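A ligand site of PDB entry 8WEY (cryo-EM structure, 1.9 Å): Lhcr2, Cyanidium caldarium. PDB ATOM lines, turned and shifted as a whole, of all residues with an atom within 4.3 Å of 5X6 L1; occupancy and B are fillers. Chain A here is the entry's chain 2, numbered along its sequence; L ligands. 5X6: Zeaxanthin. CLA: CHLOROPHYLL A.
The side-chain carboxylate (OD1) of Asp 164 lies within hydrogen-bond range of an oxygen (O08) of 5X6 L1 (3.1 Å).
The backbone NH of Leu 166 lies within hydrogen-bond range of an oxygen (O08) of 5X6 L1.
A magnesium atom (MG) of CLA L4 is bound by the side-chain amide oxygen of Gln 201 (2.5 Å).
The backbone NH (N) of Phe 163 lies within hydrogen-bond range of an oxygen (OBD) of CLA L2 (2.9 Å).
O37 of 5X6 L1 sits at hydrogen-bond distance from NE2 of Gln 201 (2.8 Å).
The side-chain carboxylate (OD1) of Asp 164 lies within hydrogen-bond range of the backbone NH (N) of Lys 167.
The backbone nitrogen (N) of Pro 165 lies close to an oxygen (O08) of 5X6 L1 (3.5 Å).
Met 90 touches 5X6 L1 (CB to C18, 3.4 Å).
Leu 91 touches 5X6 L1 (CD2 to C42, 3.9 Å).
CG1 of Val 93 touches C23 of 5X6 L1, at 3.8 Å.
CD1 of Leu 94 touches C41 of 5X6 L1 (3.5 Å).
Phe 163 touches 5X6 L1.
O of Asn 187 touches C40 of 5X6 L1, at 3.1 Å.
CD2 of Leu 190 touches C24 of 5X6 L1, 3.7 Å away.
Ala 191 touches 5X6 L1 (CB to C21, 3.8 Å).
Ala 194 touches 5X6 L1 (O to C38, 3.3 Å).
Phe 198 touches 5X6 L1.
Ile 209 touches 5X6 L1 (CG2 to C32, 3.9 Å).
Hydrophobic or aromatic side chains within 4 Å of 5X6 L1: Met 90, Leu 91, Val 93, Leu 94, Phe 163, Pro 165, Leu 166, Leu 190, Ala 191, Ala 194, Phe 198 and Ile 209.
Of the 17 residues printed, 15 come within 4 Å of 5X6 L1.
The nearest printed residue that does not touch 5X6 L1 is Leu 213 (4.04 Å).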
ATOM      1  N   MET A  90      32.097 -28.976  -6.361  1.00  0.00           N
ATOM      2  CA  MET A  90      30.838 -28.206  -6.209  1.00  0.00           C
ATOM      3  C   MET A  90      30.415 -27.601  -7.555  1.00  0.00           C
ATOM      4  O   MET A  90      29.237 -27.795  -7.931  1.00  0.00           O
ATOM      5  CB  MET A  90      30.954 -27.103  -5.158  1.00  0.00           C
ATOM      6  CG  MET A  90      30.601 -27.588  -3.773  1.00  0.00           C
ATOM      7  SD  MET A  90      30.663 -26.315  -2.491  1.00  0.00           S
ATOM      8  CE  MET A  90      32.423 -26.042  -2.341  1.00  0.00           C
ATOM      9  N   LEU A  91      31.342 -26.942  -8.251  1.00  0.00           N
ATOM     10  CA  LEU A  91      31.095 -26.378  -9.609  1.00  0.00           C
ATOM     11  C   LEU A  91      30.711 -27.513 -10.572  1.00  0.00           C
ATOM     12  O   LEU A  91      29.788 -27.317 -11.382  1.00  0.00           O
ATOM     13  CB  LEU A  91      32.352 -25.652 -10.113  1.00  0.00           C
ATOM     14  CG  LEU A  91      32.690 -24.329  -9.421  1.00  0.00           C
ATOM     15  CD1 LEU A  91      34.035 -23.819  -9.939  1.00  0.00           C
ATOM     16  CD2 LEU A  91      31.608 -23.294  -9.640  1.00  0.00           C
ATOM     17  N   VAL A  93      29.438 -30.679  -9.942  1.00  0.00           N
ATOM     18  CA  VAL A  93      28.112 -31.279  -9.584  1.00  0.00           C
ATOM     19  C   VAL A  93      26.990 -30.358 -10.110  1.00  0.00           C
ATOM     20  O   VAL A  93      26.045 -30.882 -10.722  1.00  0.00           O
ATOM     21  CB  VAL A  93      27.990 -31.518  -8.064  1.00  0.00           C
ATOM     22  CG1 VAL A  93      26.560 -31.802  -7.632  1.00  0.00           C
ATOM     23  CG2 VAL A  93      28.895 -32.652  -7.618  1.00  0.00           C
ATOM     24  N   LEU A  94      27.105 -29.049  -9.869  1.00  0.00           N
ATOM     25  CA  LEU A  94      26.127 -28.030 -10.338  1.00  0.00           C
ATOM     26  C   LEU A  94      26.190 -27.940 -11.873  1.00  0.00           C
ATOM     27  O   LEU A  94      25.124 -27.813 -12.501  1.00  0.00           O
ATOM     28  CB  LEU A  94      26.414 -26.677  -9.702  1.00  0.00           C
ATOM     29  CG  LEU A  94      25.250 -25.688  -9.780  1.00  0.00           C
ATOM     30  CD1 LEU A  94      25.215 -24.774  -8.567  1.00  0.00           C
ATOM     31  CD2 LEU A  94      25.301 -24.863 -11.046  1.00  0.00           C
ATOM     32  N   PHE A 163      38.632 -13.632  -1.453  1.00  0.00           N
ATOM     33  CA  PHE A 163      37.580 -13.353  -2.462  1.00  0.00           C
ATOM     34  C   PHE A 163      36.207 -13.364  -1.761  1.00  0.00           C
ATOM     35  O   PHE A 163      35.683 -14.462  -1.479  1.00  0.00           O
ATOM     36  CB  PHE A 163      37.602 -14.382  -3.601  1.00  0.00           C
ATOM     37  CG  PHE A 163      36.516 -14.204  -4.627  1.00  0.00           C
ATOM     38  CD1 PHE A 163      36.593 -13.177  -5.566  1.00  0.00           C
ATOM     39  CD2 PHE A 163      35.414 -15.038  -4.655  1.00  0.00           C
ATOM     40  CE1 PHE A 163      35.588 -13.003  -6.503  1.00  0.00           C
ATOM     41  CE2 PHE A 163      34.411 -14.859  -5.600  1.00  0.00           C
ATOM     42  CZ  PHE A 163      34.503 -13.852  -6.523  1.00  0.00           C
ATOM     43  N   ASP A 164      35.678 -12.172  -1.483  1.00  0.00           N
ATOM     44  CA  ASP A 164      34.299 -11.976  -0.939  1.00  0.00           C
ATOM     45  C   ASP A 164      33.796 -10.600  -1.383  1.00  0.00           C
ATOM     46  O   ASP A 164      33.612  -9.716  -0.552  1.00  0.00           O
ATOM     47  CB  ASP A 164      34.301 -12.184   0.583  1.00  0.00           C
ATOM     48  CG  ASP A 164      32.942 -12.468   1.185  1.00  0.00           C
ATOM     49  OD1 ASP A 164      31.957 -12.563   0.422  1.00  0.00           O
ATOM     50  OD2 ASP A 164      32.880 -12.616   2.420  1.00  0.00           O
ATOM     51  N   PRO A 165      33.564 -10.381  -2.702  1.00  0.00           N
ATOM     52  CA  PRO A 165      33.015  -9.118  -3.196  1.00  0.00           C
ATOM     53  C   PRO A 165      31.723  -8.661  -2.512  1.00  0.00           C
ATOM     54  O   PRO A 165      31.619  -7.481  -2.211  1.00  0.00           O
ATOM     55  CB  PRO A 165      32.718  -9.410  -4.682  1.00  0.00           C
ATOM     56  CG  PRO A 165      33.707 -10.495  -5.052  1.00  0.00           C
ATOM     57  CD  PRO A 165      33.860 -11.326  -3.794  1.00  0.00           C
ATOM     58  N   LEU A 166      30.777  -9.585  -2.291  1.00  0.00           N
ATOM     59  CA  LEU A 166      29.418  -9.305  -1.755  1.00  0.00           C
ATOM     60  C   LEU A 166      29.432  -9.270  -0.214  1.00  0.00           C
ATOM     61  O   LEU A 166      28.428  -8.807   0.350  1.00  0.00           O
ATOM     62  CB  LEU A 166      28.445 -10.373  -2.274  1.00  0.00           C
ATOM     63  CG  LEU A 166      28.245 -10.405  -3.792  1.00  0.00           C
ATOM     64  CD1 LEU A 166      27.365 -11.572  -4.189  1.00  0.00           C
ATOM     65  CD2 LEU A 166      27.672  -9.090  -4.299  1.00  0.00           C
ATOM     66  N   LYS A 167      30.508  -9.749   0.424  1.00  0.00           N
ATOM     67  CA  LYS A 167      30.681  -9.832   1.906  1.00  0.00           C
ATOM     68  C   LYS A 167      29.545 -10.686   2.489  1.00  0.00           C
ATOM     69  O   LYS A 167      28.762 -10.177   3.322  1.00  0.00           O
ATOM     70  CB  LYS A 167      30.775  -8.430   2.531  1.00  0.00           C
ATOM     71  CG  LYS A 167      32.115  -7.738   2.322  1.00  0.00           C
ATOM     72  CD  LYS A 167      32.206  -6.383   3.002  1.00  0.00           C
ATOM     73  CE  LYS A 167      31.437  -5.311   2.277  1.00  0.00           C
ATOM     74  NZ  LYS A 167      31.663  -3.965   2.871  1.00  0.00           N
ATOM     75  N   ASN A 187      29.496 -28.601   2.303  1.00  0.00           N
ATOM     76  CA  ASN A 187      28.895 -28.528   0.937  1.00  0.00           C
ATOM     77  C   ASN A 187      29.844 -29.174  -0.080  1.00  0.00           C
ATOM     78  O   ASN A 187      29.348 -29.896  -0.964  1.00  0.00           O
ATOM     79  CB  ASN A 187      28.564 -27.088   0.514  1.00  0.00           C
ATOM     80  CG  ASN A 187      27.246 -26.595   1.072  1.00  0.00           C
ATOM     81  OD1 ASN A 187      26.302 -26.395   0.316  1.00  0.00           O
ATOM     82  ND2 ASN A 187      27.183 -26.398   2.378  1.00  0.00           N
ATOM     83  N   LEU A 190      30.253 -33.052   0.331  1.00  0.00           N
ATOM     84  CA  LEU A 190      28.988 -33.659  -0.165  1.00  0.00           C
ATOM     85  C   LEU A 190      29.012 -33.720  -1.699  1.00  0.00           C
ATOM     86  O   LEU A 190      28.636 -34.777  -2.244  1.00  0.00           O
ATOM     87  CB  LEU A 190      27.804 -32.828   0.331  1.00  0.00           C
ATOM     88  CG  LEU A 190      26.408 -33.369   0.036  1.00  0.00           C
ATOM     89  CD1 LEU A 190      26.189 -34.707   0.733  1.00  0.00           C
ATOM     90  CD2 LEU A 190      25.347 -32.367   0.435  1.00  0.00           C
ATOM     91  N   ALA A 191      29.455 -32.638  -2.361  1.00  0.00           N
ATOM     92  CA  ALA A 191      29.594 -32.523  -3.827  1.00  0.00           C
ATOM     93  C   ALA A 191      30.653 -33.505  -4.333  1.00  0.00           C
ATOM     94  O   ALA A 191      30.395 -34.191  -5.346  1.00  0.00           O
ATOM     95  CB  ALA A 191      29.930 -31.106  -4.206  1.00  0.00           C
ATOM     96  N   ALA A 194      29.012 -36.838  -4.040  1.00  0.00           N
ATOM     97  CA  ALA A 194      27.865 -36.751  -4.980  1.00  0.00           C
ATOM     98  C   ALA A 194      28.338 -37.000  -6.418  1.00  0.00           C
ATOM     99  O   ALA A 194      27.662 -37.766  -7.128  1.00  0.00           O
ATOM    100  CB  ALA A 194      27.172 -35.412  -4.862  1.00  0.00           C
ATOM    101  N   PHE A 198      27.120 -39.514  -9.284  1.00  0.00           N
ATOM    102  CA  PHE A 198      26.762 -38.977 -10.626  1.00  0.00           C
ATOM    103  C   PHE A 198      27.448 -39.808 -11.719  1.00  0.00           C
ATOM    104  O   PHE A 198      26.734 -40.438 -12.528  1.00  0.00           O
ATOM    105  CB  PHE A 198      27.163 -37.499 -10.756  1.00  0.00           C
ATOM    106  CG  PHE A 198      26.188 -36.495 -10.193  1.00  0.00           C
ATOM    107  CD1 PHE A 198      25.379 -36.783  -9.100  1.00  0.00           C
ATOM    108  CD2 PHE A 198      26.111 -35.227 -10.761  1.00  0.00           C
ATOM    109  CE1 PHE A 198      24.511 -35.833  -8.598  1.00  0.00           C
ATOM    110  CE2 PHE A 198      25.240 -34.282 -10.249  1.00  0.00           C
ATOM    111  CZ  PHE A 198      24.438 -34.585  -9.174  1.00  0.00           C
ATOM    112  N   GLN A 201      26.747 -43.984 -11.606  1.00  0.00           N
ATOM    113  CA  GLN A 201      25.325 -44.296 -11.936  1.00  0.00           C
ATOM    114  C   GLN A 201      25.066 -44.081 -13.427  1.00  0.00           C
ATOM    115  O   GLN A 201      24.426 -44.954 -14.046  1.00  0.00           O
ATOM    116  CB  GLN A 201      24.381 -43.441 -11.095  1.00  0.00           C
ATOM    117  CG  GLN A 201      24.383 -43.807  -9.612  1.00  0.00           C
ATOM    118  CD  GLN A 201      23.747 -42.735  -8.761  1.00  0.00           C
ATOM    119  OE1 GLN A 201      24.123 -42.532  -7.607  1.00  0.00           O
ATOM    120  NE2 GLN A 201      22.782 -42.032  -9.330  1.00  0.00           N
ATOM    121  N   ILE A 209      21.167 -37.910 -14.744  1.00  0.00           N
ATOM    122  CA  ILE A 209      20.965 -37.896 -13.259  1.00  0.00           C
ATOM    123  C   ILE A 209      19.514 -37.508 -12.945  1.00  0.00           C
ATOM    124  O   ILE A 209      18.914 -38.154 -12.063  1.00  0.00           O
ATOM    125  CB  ILE A 209      21.978 -36.964 -12.558  1.00  0.00           C
ATOM    126  CG1 ILE A 209      23.425 -37.332 -12.862  1.00  0.00           C
ATOM    127  CG2 ILE A 209      21.730 -36.914 -11.053  1.00  0.00           C
ATOM    128  CD1 ILE A 209      23.777 -38.772 -12.586  1.00  0.00           C
ATOM    129  N   LEU A 213      16.275 -40.131 -11.840  1.00  0.00           N
ATOM    130  CA  LEU A 213      15.376 -39.759 -10.714  1.00  0.00           C
ATOM    131  C   LEU A 213      13.904 -39.884 -11.129  1.00  0.00           C
ATOM    132  O   LEU A 213      13.125 -40.488 -10.364  1.00  0.00           O
ATOM    133  CB  LEU A 213      15.687 -38.322 -10.270  1.00  0.00           C
ATOM    134  CG  LEU A 213      16.922 -38.165  -9.374  1.00  0.00           C
ATOM    135  CD1 LEU A 213      17.390 -36.712  -9.348  1.00  0.00           C
ATOM    136  CD2 LEU A 213      16.637 -38.657  -7.964  1.00  0.00           C
HETATM  137  C17 5X6 L   1      27.770 -23.920  -5.896  1.00  0.00           C
HETATM  138  C18 5X6 L   1      28.037 -25.381  -5.408  1.00  0.00           C
HETATM  139  C16 5X6 L   1      28.282 -22.891  -4.864  1.00  0.00           C
HETATM  140  C26 5X6 L   1      24.015 -34.347  -3.653  1.00  0.00           C
HETATM  141  C19 5X6 L   1      27.047 -25.958  -4.356  1.00  0.00           C
HETATM  142  C10 5X6 L   1      30.324 -15.206  -6.698  1.00  0.00           C
HETATM  143  C11 5X6 L   1      30.313 -17.821  -4.821  1.00  0.00           C
HETATM  144  C12 5X6 L   1      30.890 -18.613  -6.014  1.00  0.00           C
HETATM  145  C13 5X6 L   1      29.902 -19.690  -6.542  1.00  0.00           C
HETATM  146  C20 5X6 L   1      26.422 -27.332  -4.753  1.00  0.00           C
HETATM  147  C14 5X6 L   1      29.821 -20.943  -5.610  1.00  0.00           C
HETATM  148  C15 5X6 L   1      28.375 -21.402  -5.325  1.00  0.00           C
HETATM  149  C35 5X6 L   1      20.554 -36.216  -6.411  1.00  0.00           C
HETATM  150  C34 5X6 L   1      20.797 -37.527  -5.637  1.00  0.00           C
HETATM  151  C33 5X6 L   1      20.427 -38.752  -6.576  1.00  0.00           C
HETATM  152  C40 5X6 L   1      26.360 -29.577  -1.858  1.00  0.00           C
HETATM  153  C32 5X6 L   1      21.408 -38.936  -7.788  1.00  0.00           C
HETATM  154  C31 5X6 L   1      22.856 -39.108  -7.296  1.00  0.00           C
HETATM  155  C30 5X6 L   1      23.243 -38.064  -6.288  1.00  0.00           C
HETATM  156  C29 5X6 L   1      22.267 -37.643  -5.260  1.00  0.00           C
HETATM  157  C39 5X6 L   1      23.508 -34.458  -2.210  1.00  0.00           C
HETATM  158  C28 5X6 L   1      22.759 -36.605  -4.182  1.00  0.00           C
HETATM  159  C27 5X6 L   1      23.228 -35.207  -4.700  1.00  0.00           C
HETATM  160  C21 5X6 L   1      27.062 -28.577  -4.098  1.00  0.00           C
HETATM  161  C36 5X6 L   1      19.902 -37.567  -4.384  1.00  0.00           C
HETATM  162  C22 5X6 L   1      26.055 -29.505  -3.346  1.00  0.00           C
HETATM  163  C23 5X6 L   1      25.913 -30.896  -4.036  1.00  0.00           C
HETATM  164  C24 5X6 L   1      25.116 -31.974  -3.242  1.00  0.00           C
HETATM  165  C25 5X6 L   1      24.259 -32.896  -4.154  1.00  0.00           C
HETATM  166  C38 5X6 L   1      24.683 -38.241  -5.800  1.00  0.00           C
HETATM  167  C01 5X6 L   1      32.906 -17.203  -3.285  1.00  0.00           C
HETATM  168  C02 5X6 L   1      31.662 -16.308  -3.354  1.00  0.00           C
HETATM  169  C03 5X6 L   1      30.959 -16.424  -4.639  1.00  0.00           C
HETATM  170  C04 5X6 L   1      30.106 -15.281  -5.184  1.00  0.00           C
HETATM  171  C05 5X6 L   1      30.541 -13.897  -4.562  1.00  0.00           C
HETATM  172  C06 5X6 L   1      30.746 -13.989  -3.017  1.00  0.00           C
HETATM  173  C07 5X6 L   1      31.917 -14.956  -2.750  1.00  0.00           C
HETATM  174  O08 5X6 L   1      31.039 -12.753  -2.490  1.00  0.00           O
HETATM  175  C09 5X6 L   1      28.609 -15.503  -4.899  1.00  0.00           C
HETATM  176  O37 5X6 L   1      21.048 -40.028  -8.547  1.00  0.00           O
HETATM  177  C41 5X6 L   1      28.323 -23.687  -7.319  1.00  0.00           C
HETATM  178  C42 5X6 L   1      30.124 -20.046  -8.022  1.00  0.00           C
HETATM  179 MG   CLA L   2      33.890 -20.590  -1.197  1.00  0.00          MG
HETATM  180  CHA CLA L   2      36.033 -18.115  -0.109  1.00  0.00           C
HETATM  181  CHB CLA L   2      32.177 -20.212   1.707  1.00  0.00           C
HETATM  182  CHC CLA L   2      31.578 -22.666  -2.496  1.00  0.00           C
HETATM  183  CHD CLA L   2      35.685 -20.500  -4.431  1.00  0.00           C
HETATM  184  NA  CLA L   2      34.030 -19.372   0.473  1.00  0.00           N
HETATM  185  C1A CLA L   2      34.919 -18.517   0.797  1.00  0.00           C
HETATM  186  C2A CLA L   2      34.776 -17.830   2.115  1.00  0.00           C
HETATM  187  C3A CLA L   2      33.613 -18.586   2.733  1.00  0.00           C
HETATM  188  C4A CLA L   2      33.258 -19.455   1.559  1.00  0.00           C
HETATM  189  CMA CLA L   2      34.107 -19.411   3.918  1.00  0.00           C
HETATM  190  CAA CLA L   2      34.294 -16.372   1.908  1.00  0.00           C
HETATM  191  CBA CLA L   2      33.337 -16.065   0.729  1.00  0.00           C
HETATM  192  CGA CLA L   2      31.898 -16.549   0.828  1.00  0.00           C
HETATM  193  O1A CLA L   2      31.268 -16.478   1.871  1.00  0.00           O
HETATM  194  O2A CLA L   2      31.235 -17.071  -0.377  1.00  0.00           O
HETATM  195  NB  CLA L   2      32.123 -21.343  -0.488  1.00  0.00           N
HETATM  196  C1B CLA L   2      31.609 -21.129   0.721  1.00  0.00           C
HETATM  197  C2B CLA L   2      30.338 -21.831   1.002  1.00  0.00           C
HETATM  198  C3B CLA L   2      30.122 -22.585  -0.260  1.00  0.00           C
HETATM  199  C4B CLA L   2      31.307 -22.195  -1.118  1.00  0.00           C
HETATM  200  CMB CLA L   2      29.457 -21.823   2.226  1.00  0.00           C
HETATM  201  CAB CLA L   2      28.918 -23.450  -0.437  1.00  0.00           C
HETATM  202  CBB CLA L   2      28.519 -24.014  -1.560  1.00  0.00           C
HETATM  203  NC  CLA L   2      33.680 -21.384  -3.073  1.00  0.00           N
HETATM  204  C1C CLA L   2      32.684 -22.249  -3.383  1.00  0.00           C
HETATM  205  C2C CLA L   2      32.784 -22.784  -4.782  1.00  0.00           C
HETATM  206  C3C CLA L   2      33.992 -22.139  -5.320  1.00  0.00           C
HETATM  207  C4C CLA L   2      34.449 -21.303  -4.197  1.00  0.00           C
HETATM  208  CMC CLA L   2      31.910 -23.747  -5.533  1.00  0.00           C
HETATM  209  CAC CLA L   2      34.597 -22.276  -6.697  1.00  0.00           C
HETATM  210  CBC CLA L   2      34.225 -21.025  -7.479  1.00  0.00           C
HETATM  211  ND  CLA L   2      35.407 -19.588  -2.137  1.00  0.00           N
HETATM  212  C1D CLA L   2      36.149 -19.629  -3.357  1.00  0.00           C
HETATM  213  C2D CLA L   2      37.359 -18.769  -3.427  1.00  0.00           C
HETATM  214  C3D CLA L   2      37.292 -18.151  -2.079  1.00  0.00           C
HETATM  215  C4D CLA L   2      36.175 -18.677  -1.441  1.00  0.00           C
HETATM  216  CMD CLA L   2      38.430 -18.469  -4.445  1.00  0.00           C
HETATM  217  CAD CLA L   2      37.933 -17.218  -1.124  1.00  0.00           C
HETATM  218  OBD CLA L   2      39.002 -16.536  -1.351  1.00  0.00           O
HETATM  219  CBD CLA L   2      37.156 -17.177   0.133  1.00  0.00           C
HETATM  220  CGD CLA L   2      38.055 -17.626   1.243  1.00  0.00           C
HETATM  221  O1D CLA L   2      38.887 -16.838   1.667  1.00  0.00           O
HETATM  222  O2D CLA L   2      37.944 -18.972   1.789  1.00  0.00           O
HETATM  223  CED CLA L   2      38.377 -19.308   3.108  1.00  0.00           C
HETATM  224  C1  CLA L   2      30.289 -18.153  -0.394  1.00  0.00           C
HETATM  225  C2  CLA L   2      29.101 -17.814  -1.277  1.00  0.00           C
HETATM  226  C3  CLA L   2      27.927 -18.479  -1.267  1.00  0.00           C
HETATM  227  C4  CLA L   2      27.628 -19.637  -0.351  1.00  0.00           C
HETATM  228  C5  CLA L   2      26.812 -18.066  -2.195  1.00  0.00           C
HETATM  229  C6  CLA L   2      26.754 -18.933  -3.454  1.00  0.00           C
HETATM  230  C7  CLA L   2      25.343 -19.086  -4.032  1.00  0.00           C
HETATM  231  C8  CLA L   2      25.120 -18.409  -5.391  1.00  0.00           C
HETATM  232  C9  CLA L   2      25.877 -19.105  -6.521  1.00  0.00           C
HETATM  233  C10 CLA L   2      25.457 -16.922  -5.311  1.00  0.00           C
HETATM  234 MG   CLA L   3      23.698 -26.460   0.610  1.00  0.00          MG
HETATM  235  CHA CLA L   3      23.794 -24.878   3.693  1.00  0.00           C
HETATM  236  CHB CLA L   3      24.571 -23.506  -0.813  1.00  0.00           C
HETATM  237  CHC CLA L   3      23.053 -27.915  -2.383  1.00  0.00           C
HETATM  238  CHD CLA L   3      22.337 -29.442   2.334  1.00  0.00           C
HETATM  239  NA  CLA L   3      24.072 -24.534   1.289  1.00  0.00           N
HETATM  240  C1A CLA L   3      24.189 -24.078   2.491  1.00  0.00           C
HETATM  241  C2A CLA L   3      24.647 -22.645   2.667  1.00  0.00           C
HETATM  242  C3A CLA L   3      24.894 -22.249   1.218  1.00  0.00           C
HETATM  243  C4A CLA L   3      24.489 -23.516   0.516  1.00  0.00           C
HETATM  244  CMA CLA L   3      24.028 -21.043   0.809  1.00  0.00           C
HETATM  245  CAA CLA L   3      25.862 -22.429   3.579  1.00  0.00           C
HETATM  246  CBA CLA L   3      26.895 -23.543   3.520  1.00  0.00           C
HETATM  247  NB  CLA L   3      23.815 -25.806  -1.328  1.00  0.00           N
HETATM  248  C1B CLA L   3      24.219 -24.603  -1.735  1.00  0.00           C
HETATM  249  C2B CLA L   3      24.216 -24.402  -3.203  1.00  0.00           C
HETATM  250  C3B CLA L   3      23.743 -25.712  -3.702  1.00  0.00           C
HETATM  251  C4B CLA L   3      23.537 -26.514  -2.440  1.00  0.00           C
HETATM  252  CMB CLA L   3      24.592 -23.181  -4.006  1.00  0.00           C
HETATM  253  CAB CLA L   3      23.585 -26.022  -5.161  1.00  0.00           C
HETATM  254  CBB CLA L   3      23.181 -27.151  -5.718  1.00  0.00           C
HETATM  255  NC  CLA L   3      22.886 -28.294   0.112  1.00  0.00           N
HETATM  256  C1C CLA L   3      22.715 -28.686  -1.174  1.00  0.00           C
HETATM  257  C2C CLA L   3      22.097 -30.040  -1.336  1.00  0.00           C
HETATM  258  C3C CLA L   3      21.901 -30.506   0.053  1.00  0.00           C
HETATM  259  C4C CLA L   3      22.422 -29.352   0.852  1.00  0.00           C
HETATM  260  CMC CLA L   3      21.758 -30.789  -2.592  1.00  0.00           C
HETATM  261  CAC CLA L   3      21.263 -31.818   0.504  1.00  0.00           C
HETATM  262  CBC CLA L   3      22.147 -32.638   1.419  1.00  0.00           C
HETATM  263  ND  CLA L   3      23.151 -27.089   2.473  1.00  0.00           N
HETATM  264  C1D CLA L   3      22.673 -28.264   3.134  1.00  0.00           C
HETATM  265  C2D CLA L   3      22.520 -28.167   4.607  1.00  0.00           C
HETATM  266  C3D CLA L   3      22.981 -26.768   4.812  1.00  0.00           C
HETATM  267  C4D CLA L   3      23.311 -26.259   3.574  1.00  0.00           C
HETATM  268  CMD CLA L   3      22.071 -29.076   5.724  1.00  0.00           C
HETATM  269  CAD CLA L   3      23.234 -25.700   5.821  1.00  0.00           C
HETATM  270  OBD CLA L   3      23.047 -25.828   7.093  1.00  0.00           O
HETATM  271  CBD CLA L   3      23.738 -24.492   5.127  1.00  0.00           C
HETATM  272  CGD CLA L   3      22.797 -23.341   5.370  1.00  0.00           C
HETATM  273  O1D CLA L   3      21.663 -23.343   4.922  1.00  0.00           O
HETATM  274  O2D CLA L   3      23.256 -22.187   6.141  1.00  0.00           O
HETATM  275  CED CLA L   3      22.623 -21.837   7.371  1.00  0.00           C
HETATM  276 MG   CLA L   4      24.734 -43.976  -5.723  1.00  0.00          MG
HETATM  277  CHA CLA L   4      22.893 -46.457  -7.297  1.00  0.00           C
HETATM  278  CHB CLA L   4      21.826 -42.803  -4.402  1.00  0.00           C
HETATM  279  CHC CLA L   4      26.621 -41.855  -3.879  1.00  0.00           C
HETATM  280  CHD CLA L   4      27.789 -45.661  -6.947  1.00  0.00           C
HETATM  281  NA  CLA L   4      22.732 -44.537  -5.790  1.00  0.00           N
HETATM  282  C1A CLA L   4      22.145 -45.452  -6.476  1.00  0.00           C
HETATM  283  C2A CLA L   4      20.640 -45.513  -6.410  1.00  0.00           C
HETATM  284  C3A CLA L   4      20.328 -44.320  -5.502  1.00  0.00           C
HETATM  285  C4A CLA L   4      21.723 -43.857  -5.214  1.00  0.00           C
HETATM  286  CMA CLA L   4      19.506 -43.261  -6.235  1.00  0.00           C
HETATM  287  CAA CLA L   4      20.097 -46.808  -5.784  1.00  0.00           C
HETATM  288  CBA CLA L   4      20.901 -47.298  -4.581  1.00  0.00           C
HETATM  289  CGA CLA L   4      20.129 -48.302  -3.752  1.00  0.00           C
HETATM  290  O1A CLA L   4      19.290 -49.035  -4.240  1.00  0.00           O
HETATM  291  O2A CLA L   4      20.394 -48.399  -2.323  1.00  0.00           O
HETATM  292  NB  CLA L   4      24.293 -42.548  -4.324  1.00  0.00           N
HETATM  293  C1B CLA L   4      23.070 -42.154  -3.960  1.00  0.00           C
HETATM  294  C2B CLA L   4      23.018 -40.978  -3.052  1.00  0.00           C
HETATM  295  C3B CLA L   4      24.453 -40.671  -2.874  1.00  0.00           C
HETATM  296  C4B CLA L   4      25.159 -41.716  -3.716  1.00  0.00           C
HETATM  297  CMB CLA L   4      21.827 -40.279  -2.455  1.00  0.00           C
HETATM  298  CAB CLA L   4      24.909 -39.516  -2.033  1.00  0.00           C
HETATM  299  CBB CLA L   4      26.138 -39.060  -1.921  1.00  0.00           C
HETATM  300  NC  CLA L   4      26.766 -43.848  -5.442  1.00  0.00           N
HETATM  301  C1C CLA L   4      27.334 -42.859  -4.709  1.00  0.00           C
HETATM  302  C2C CLA L   4      28.824 -42.813  -4.799  1.00  0.00           C
HETATM  303  C3C CLA L   4      29.162 -43.939  -5.687  1.00  0.00           C
HETATM  304  C4C CLA L   4      27.829 -44.493  -6.032  1.00  0.00           C
HETATM  305  CMC CLA L   4      29.819 -41.893  -4.145  1.00  0.00           C
HETATM  306  CAC CLA L   4      30.546 -44.368  -6.157  1.00  0.00           C
HETATM  307  CBC CLA L   4      30.938 -45.721  -5.614  1.00  0.00           C
HETATM  308  ND  CLA L   4      25.297 -45.632  -6.784  1.00  0.00           N
HETATM  309  C1D CLA L   4      26.489 -46.219  -7.320  1.00  0.00           C
HETATM  310  C2D CLA L   4      26.296 -47.380  -8.225  1.00  0.00           C
HETATM  311  C3D CLA L   4      24.808 -47.462  -8.212  1.00  0.00           C
HETATM  312  C4D CLA L   4      24.360 -46.447  -7.378  1.00  0.00           C
HETATM  313  CMD CLA L   4      27.180 -48.312  -9.017  1.00  0.00           C
HETATM  314  CAD CLA L   4      23.622 -48.189  -8.717  1.00  0.00           C
HETATM  315  OBD CLA L   4      23.649 -49.200  -9.506  1.00  0.00           O
HETATM  316  CBD CLA L   4      22.395 -47.574  -8.151  1.00  0.00           C
HETATM  317  CGD CLA L   4      21.506 -47.079  -9.257  1.00  0.00           C
HETATM  318  O1D CLA L   4      21.921 -46.343 -10.139  1.00  0.00           O
HETATM  319  O2D CLA L   4      20.108 -47.496  -9.298  1.00  0.00           O
HETATM  320  CED CLA L   4      19.569 -48.149 -10.448  1.00  0.00           C
